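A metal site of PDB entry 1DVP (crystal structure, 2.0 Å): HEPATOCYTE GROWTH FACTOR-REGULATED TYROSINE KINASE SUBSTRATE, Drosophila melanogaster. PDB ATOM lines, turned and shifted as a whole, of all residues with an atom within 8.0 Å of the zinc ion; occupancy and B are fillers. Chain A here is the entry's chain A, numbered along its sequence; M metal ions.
Four residues have an atom within 4 Å of the zinc ion: Cys 180, Cys 183, Cys 210 and Cys 213. The nearest printed residue that does not touch the zinc ion is Phe 187 (4.01 Å).
SG of Cys 180 binds the zinc ion (2.3 Å). SG of Cys 183 is bound to the zinc ion, at 2.4 Å. The zinc ion is bound by the side-chain sulfur (SG) of Cys 213 (2.4 Å). The zinc ion is bound by SG of Cys 210.
N of Gly 212 lies close to SG of Cys 210, at 3.7 Å. The backbone NH of Gln 185 sits close to the side-chain sulfur of Cys 183, at 3.7 Å. The side-chain amide oxygen (OD1) of Asn 182 lies close to the side-chain sulfur (SG) of Cys 213 (3.3 Å). The side-chain sulfur of Cys 180 sits close to the backbone NH of Asn 182, 3.3 Å away. The backbone carbonyl oxygen of Gln 185 is in hydrogen-bond range of the backbone NH of Cys 180 (3.0 Å).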
ATOM      1  N   PRO A 156     -21.765  -2.878 -17.854  1.00  0.00           N
ATOM      2  CA  PRO A 156     -23.120  -3.295 -17.450  1.00  0.00           C
ATOM      3  C   PRO A 156     -23.014  -4.367 -16.343  1.00  0.00           C
ATOM      4  O   PRO A 156     -21.963  -5.033 -16.225  1.00  0.00           O
ATOM      5  CB  PRO A 156     -23.666  -3.898 -18.718  1.00  0.00           C
ATOM      6  CG  PRO A 156     -22.456  -4.704 -19.180  1.00  0.00           C
ATOM      7  CD  PRO A 156     -21.345  -3.627 -19.049  1.00  0.00           C
ATOM      8  N   HIS A 165     -27.534 -16.789 -23.774  1.00  0.00           N
ATOM      9  CA  HIS A 165     -28.360 -15.688 -24.293  1.00  0.00           C
ATOM     10  C   HIS A 165     -28.501 -15.683 -25.835  1.00  0.00           C
ATOM     11  O   HIS A 165     -29.571 -15.375 -26.375  1.00  0.00           O
ATOM     12  CB  HIS A 165     -27.744 -14.354 -23.849  1.00  0.00           C
ATOM     13  CG  HIS A 165     -28.591 -13.147 -24.151  1.00  0.00           C
ATOM     14  ND1 HIS A 165     -29.820 -12.930 -23.563  1.00  0.00           N
ATOM     15  CD2 HIS A 165     -28.370 -12.082 -24.964  1.00  0.00           C
ATOM     16  CE1 HIS A 165     -30.328 -11.796 -23.996  1.00  0.00           C
ATOM     17  NE2 HIS A 165     -29.470 -11.261 -24.849  1.00  0.00           N
ATOM     18  N   ARG A 166     -27.429 -16.015 -26.526  1.00  0.00           N
ATOM     19  CA  ARG A 166     -27.473 -15.984 -27.959  1.00  0.00           C
ATOM     20  C   ARG A 166     -28.071 -17.202 -28.646  1.00  0.00           C
ATOM     21  O   ARG A 166     -29.077 -17.092 -29.378  1.00  0.00           O
ATOM     22  CB  ARG A 166     -26.057 -15.685 -28.550  1.00  0.00           C
ATOM     23  CG  ARG A 166     -26.048 -15.388 -30.087  1.00  0.00           C
ATOM     24  CD  ARG A 166     -24.621 -15.100 -30.578  1.00  0.00           C
ATOM     25  NE  ARG A 166     -24.473 -14.628 -31.982  1.00  0.00           N
ATOM     26  CZ  ARG A 166     -24.756 -13.388 -32.425  1.00  0.00           C
ATOM     27  NH1 ARG A 166     -25.258 -12.443 -31.624  1.00  0.00           N
ATOM     28  NH2 ARG A 166     -24.445 -13.063 -33.670  1.00  0.00           N
ATOM     29  N   HIS A 179     -19.560 -14.790 -18.810  1.00  0.00           N
ATOM     30  CA  HIS A 179     -20.176 -13.510 -19.083  1.00  0.00           C
ATOM     31  C   HIS A 179     -19.409 -12.732 -20.170  1.00  0.00           C
ATOM     32  O   HIS A 179     -18.158 -12.780 -20.268  1.00  0.00           O
ATOM     33  CB  HIS A 179     -20.220 -12.604 -17.810  1.00  0.00           C
ATOM     34  CG  HIS A 179     -21.106 -13.127 -16.730  1.00  0.00           C
ATOM     35  ND1 HIS A 179     -20.742 -14.169 -15.893  1.00  0.00           N
ATOM     36  CD2 HIS A 179     -22.346 -12.746 -16.338  1.00  0.00           C
ATOM     37  CE1 HIS A 179     -21.719 -14.412 -15.035  1.00  0.00           C
ATOM     38  NE2 HIS A 179     -22.700 -13.556 -15.288  1.00  0.00           N
ATOM     39  N   CYS A 180     -20.172 -12.038 -21.002  1.00  0.00           N
ATOM     40  CA  CYS A 180     -19.617 -11.135 -21.996  1.00  0.00           C
ATOM     41  C   CYS A 180     -19.270  -9.874 -21.158  1.00  0.00           C
ATOM     42  O   CYS A 180     -20.135  -9.330 -20.469  1.00  0.00           O
ATOM     43  CB  CYS A 180     -20.679 -10.698 -23.006  1.00  0.00           C
ATOM     44  SG  CYS A 180     -20.182  -9.362 -24.126  1.00  0.00           S
ATOM     45  N   ARG A 181     -18.071  -9.383 -21.277  1.00  0.00           N
ATOM     46  CA  ARG A 181     -17.713  -8.169 -20.532  1.00  0.00           C
ATOM     47  C   ARG A 181     -18.305  -6.880 -21.118  1.00  0.00           C
ATOM     48  O   ARG A 181     -18.264  -5.860 -20.452  1.00  0.00           O
ATOM     49  CB  ARG A 181     -16.195  -8.039 -20.469  1.00  0.00           C
ATOM     50  CG  ARG A 181     -15.588  -8.850 -19.419  1.00  0.00           C
ATOM     51  CD  ARG A 181     -15.720 -10.320 -19.630  1.00  0.00           C
ATOM     52  NE  ARG A 181     -14.832 -11.008 -18.687  1.00  0.00           N
ATOM     53  CZ  ARG A 181     -14.873 -12.291 -18.374  1.00  0.00           C
ATOM     54  NH1 ARG A 181     -15.763 -13.146 -18.884  1.00  0.00           N
ATOM     55  NH2 ARG A 181     -13.971 -12.731 -17.487  1.00  0.00           N
ATOM     56  N   ASN A 182     -18.838  -6.891 -22.345  1.00  0.00           N
ATOM     57  CA  ASN A 182     -19.463  -5.697 -22.905  1.00  0.00           C
ATOM     58  C   ASN A 182     -20.938  -5.563 -22.537  1.00  0.00           C
ATOM     59  O   ASN A 182     -21.391  -4.450 -22.205  1.00  0.00           O
ATOM     60  CB  ASN A 182     -19.369  -5.654 -24.447  1.00  0.00           C
ATOM     61  CG  ASN A 182     -19.753  -4.277 -25.017  1.00  0.00           C
ATOM     62  OD1 ASN A 182     -20.618  -4.168 -25.905  1.00  0.00           O
ATOM     63  ND2 ASN A 182     -19.127  -3.222 -24.491  1.00  0.00           N
ATOM     64  N   CYS A 183     -21.727  -6.645 -22.582  1.00  0.00           N
ATOM     65  CA  CYS A 183     -23.171  -6.486 -22.265  1.00  0.00           C
ATOM     66  C   CYS A 183     -23.574  -7.136 -20.958  1.00  0.00           C
ATOM     67  O   CYS A 183     -24.691  -6.972 -20.510  1.00  0.00           O
ATOM     68  CB  CYS A 183     -24.059  -7.031 -23.403  1.00  0.00           C
ATOM     69  SG  CYS A 183     -23.925  -8.831 -23.762  1.00  0.00           S
ATOM     70  N   GLY A 184     -22.671  -7.904 -20.361  1.00  0.00           N
ATOM     71  CA  GLY A 184     -22.994  -8.543 -19.077  1.00  0.00           C
ATOM     72  C   GLY A 184     -23.873  -9.793 -19.119  1.00  0.00           C
ATOM     73  O   GLY A 184     -24.151 -10.373 -18.088  1.00  0.00           O
ATOM     74  N   GLN A 185     -24.352 -10.214 -20.306  1.00  0.00           N
ATOM     75  CA  GLN A 185     -25.173 -11.447 -20.379  1.00  0.00           C
ATOM     76  C   GLN A 185     -24.286 -12.686 -20.252  1.00  0.00           C
ATOM     77  O   GLN A 185     -23.047 -12.560 -20.402  1.00  0.00           O
ATOM     78  CB  GLN A 185     -25.921 -11.529 -21.715  1.00  0.00           C
ATOM     79  CG  GLN A 185     -27.258 -10.766 -21.624  1.00  0.00           C
ATOM     80  CD  GLN A 185     -28.235 -11.523 -20.723  1.00  0.00           C
ATOM     81  OE1 GLN A 185     -28.009 -12.712 -20.293  1.00  0.00           O
ATOM     82  NE2 GLN A 185     -29.311 -10.888 -20.456  1.00  0.00           N
ATOM     83  N   VAL A 186     -24.925 -13.859 -20.051  1.00  0.00           N
ATOM     84  CA  VAL A 186     -24.218 -15.143 -19.919  1.00  0.00           C
ATOM     85  C   VAL A 186     -24.459 -15.822 -21.256  1.00  0.00           C
ATOM     86  O   VAL A 186     -25.547 -15.669 -21.814  1.00  0.00           O
ATOM     87  CB  VAL A 186     -24.748 -16.100 -18.784  1.00  0.00           C
ATOM     88  CG1 VAL A 186     -24.275 -15.583 -17.393  1.00  0.00           C
ATOM     89  CG2 VAL A 186     -26.237 -16.151 -18.814  1.00  0.00           C
ATOM     90  N   PHE A 187     -23.420 -16.521 -21.716  1.00  0.00           N
ATOM     91  CA  PHE A 187     -23.355 -17.244 -22.983  1.00  0.00           C
ATOM     92  C   PHE A 187     -22.495 -18.495 -22.804  1.00  0.00           C
ATOM     93  O   PHE A 187     -21.727 -18.626 -21.806  1.00  0.00           O
ATOM     94  CB  PHE A 187     -22.631 -16.391 -24.052  1.00  0.00           C
ATOM     95  CG  PHE A 187     -23.222 -15.006 -24.257  1.00  0.00           C
ATOM     96  CD1 PHE A 187     -22.955 -13.941 -23.371  1.00  0.00           C
ATOM     97  CD2 PHE A 187     -24.033 -14.747 -25.365  1.00  0.00           C
ATOM     98  CE1 PHE A 187     -23.484 -12.650 -23.587  1.00  0.00           C
ATOM     99  CE2 PHE A 187     -24.563 -13.492 -25.593  1.00  0.00           C
ATOM    100  CZ  PHE A 187     -24.285 -12.417 -24.679  1.00  0.00           C
ATOM    101  N   CYS A 191     -20.285 -19.124 -28.056  1.00  0.00           N
ATOM    102  CA  CYS A 191     -20.795 -17.810 -28.454  1.00  0.00           C
ATOM    103  C   CYS A 191     -19.956 -16.634 -27.887  1.00  0.00           C
ATOM    104  O   CYS A 191     -20.291 -15.497 -28.134  1.00  0.00           O
ATOM    105  CB  CYS A 191     -22.255 -17.620 -28.015  1.00  0.00           C
ATOM    106  SG  CYS A 191     -23.447 -18.618 -29.029  1.00  0.00           S
ATOM    107  N   THR A 192     -18.899 -16.932 -27.139  1.00  0.00           N
ATOM    108  CA  THR A 192     -18.008 -15.918 -26.537  1.00  0.00           C
ATOM    109  C   THR A 192     -16.550 -16.385 -26.681  1.00  0.00           C
ATOM    110  O   THR A 192     -15.768 -16.326 -25.733  1.00  0.00           O
ATOM    111  CB  THR A 192     -18.320 -15.704 -24.978  1.00  0.00           C
ATOM    112  OG1 THR A 192     -18.474 -16.972 -24.314  1.00  0.00           O
ATOM    113  CG2 THR A 192     -19.561 -14.924 -24.840  1.00  0.00           C
ATOM    114  N   ARG A 208     -13.107 -11.413 -22.825  1.00  0.00           N
ATOM    115  CA  ARG A 208     -14.154 -12.196 -23.493  1.00  0.00           C
ATOM    116  C   ARG A 208     -15.406 -11.340 -23.841  1.00  0.00           C
ATOM    117  O   ARG A 208     -15.852 -10.602 -22.999  1.00  0.00           O
ATOM    118  CB  ARG A 208     -14.556 -13.351 -22.554  1.00  0.00           C
ATOM    119  CG  ARG A 208     -15.764 -14.172 -23.066  1.00  0.00           C
ATOM    120  CD  ARG A 208     -16.309 -15.070 -21.984  1.00  0.00           C
ATOM    121  NE  ARG A 208     -15.282 -15.975 -21.506  1.00  0.00           N
ATOM    122  CZ  ARG A 208     -14.903 -17.102 -22.109  1.00  0.00           C
ATOM    123  NH1 ARG A 208     -15.478 -17.476 -23.228  1.00  0.00           N
ATOM    124  NH2 ARG A 208     -13.969 -17.844 -21.562  1.00  0.00           N
ATOM    125  N   VAL A 209     -15.910 -11.414 -25.102  1.00  0.00           N
ATOM    126  CA  VAL A 209     -17.134 -10.715 -25.490  1.00  0.00           C
ATOM    127  C   VAL A 209     -18.036 -11.717 -26.319  1.00  0.00           C
ATOM    128  O   VAL A 209     -17.551 -12.676 -26.877  1.00  0.00           O
ATOM    129  CB  VAL A 209     -16.876  -9.471 -26.370  1.00  0.00           C
ATOM    130  CG1 VAL A 209     -16.179  -8.367 -25.545  1.00  0.00           C
ATOM    131  CG2 VAL A 209     -15.993  -9.800 -27.549  1.00  0.00           C
ATOM    132  N   CYS A 210     -19.330 -11.472 -26.372  1.00  0.00           N
ATOM    133  CA  CYS A 210     -20.219 -12.319 -27.166  1.00  0.00           C
ATOM    134  C   CYS A 210     -20.153 -11.851 -28.650  1.00  0.00           C
ATOM    135  O   CYS A 210     -19.665 -10.755 -28.988  1.00  0.00           O
ATOM    136  CB  CYS A 210     -21.662 -12.206 -26.632  1.00  0.00           C
ATOM    137  SG  CYS A 210     -22.431 -10.680 -27.067  1.00  0.00           S
ATOM    138  N   ASP A 211     -20.680 -12.700 -29.520  1.00  0.00           N
ATOM    139  CA  ASP A 211     -20.685 -12.438 -30.953  1.00  0.00           C
ATOM    140  C   ASP A 211     -21.427 -11.173 -31.301  1.00  0.00           C
ATOM    141  O   ASP A 211     -20.920 -10.394 -32.044  1.00  0.00           O
ATOM    142  CB  ASP A 211     -21.249 -13.668 -31.689  1.00  0.00           C
ATOM    143  CG  ASP A 211     -20.245 -14.786 -31.707  1.00  0.00           C
ATOM    144  OD1 ASP A 211     -19.074 -14.480 -31.510  1.00  0.00           O
ATOM    145  OD2 ASP A 211     -20.581 -15.966 -31.909  1.00  0.00           O
ATOM    146  N   GLY A 212     -22.605 -10.958 -30.751  1.00  0.00           N
ATOM    147  CA  GLY A 212     -23.337  -9.736 -31.042  1.00  0.00           C
ATOM    148  C   GLY A 212     -22.537  -8.475 -30.704  1.00  0.00           C
ATOM    149  O   GLY A 212     -22.518  -7.522 -31.501  1.00  0.00           O
ATOM    150  N   CYS A 213     -21.908  -8.455 -29.520  1.00  0.00           N
ATOM    151  CA  CYS A 213     -21.071  -7.306 -29.068  1.00  0.00           C
ATOM    152  C   CYS A 213     -19.812  -7.168 -29.919  1.00  0.00           C
ATOM    153  O   CYS A 213     -19.444  -6.077 -30.287  1.00  0.00           O
ATOM    154  CB  CYS A 213     -20.693  -7.446 -27.568  1.00  0.00           C
ATOM    155  SG  CYS A 213     -22.132  -7.065 -26.531  1.00  0.00           S
ATOM    156  N   PHE A 214     -19.150  -8.270 -30.217  1.00  0.00           N
ATOM    157  CA  PHE A 214     -17.953  -8.198 -31.051  1.00  0.00           C
ATOM    158  C   PHE A 214     -18.286  -7.577 -32.409  1.00  0.00           C
ATOM    159  O   PHE A 214     -17.477  -6.839 -32.999  1.00  0.00           O
ATOM    160  CB  PHE A 214     -17.413  -9.587 -31.302  1.00  0.00           C
ATOM    161  CG  PHE A 214     -16.181  -9.612 -32.131  1.00  0.00           C
ATOM    162  CD1 PHE A 214     -14.948  -9.474 -31.552  1.00  0.00           C
ATOM    163  CD2 PHE A 214     -16.265  -9.771 -33.528  1.00  0.00           C
ATOM    164  CE1 PHE A 214     -13.803  -9.512 -32.311  1.00  0.00           C
ATOM    165  CE2 PHE A 214     -15.129  -9.805 -34.314  1.00  0.00           C
ATOM    166  CZ  PHE A 214     -13.896  -9.677 -33.699  1.00  0.00           C
ATOM    167  N   LEU A 217     -19.173  -3.692 -31.724  1.00  0.00           N
ATOM    168  CA  LEU A 217     -17.946  -2.988 -31.364  1.00  0.00           C
ATOM    169  C   LEU A 217     -17.091  -2.788 -32.611  1.00  0.00           C
ATOM    170  O   LEU A 217     -16.375  -1.814 -32.746  1.00  0.00           O
ATOM    171  CB  LEU A 217     -17.132  -3.796 -30.341  1.00  0.00           C
ATOM    172  CG  LEU A 217     -17.540  -3.700 -28.860  1.00  0.00           C
ATOM    173  CD1 LEU A 217     -16.775  -4.734 -28.057  1.00  0.00           C
ATOM    174  CD2 LEU A 217     -17.269  -2.269 -28.286  1.00  0.00           C
HETATM  175 ZN    ZN M   1     -22.152  -9.081 -25.288  1.00  0.00          ZN
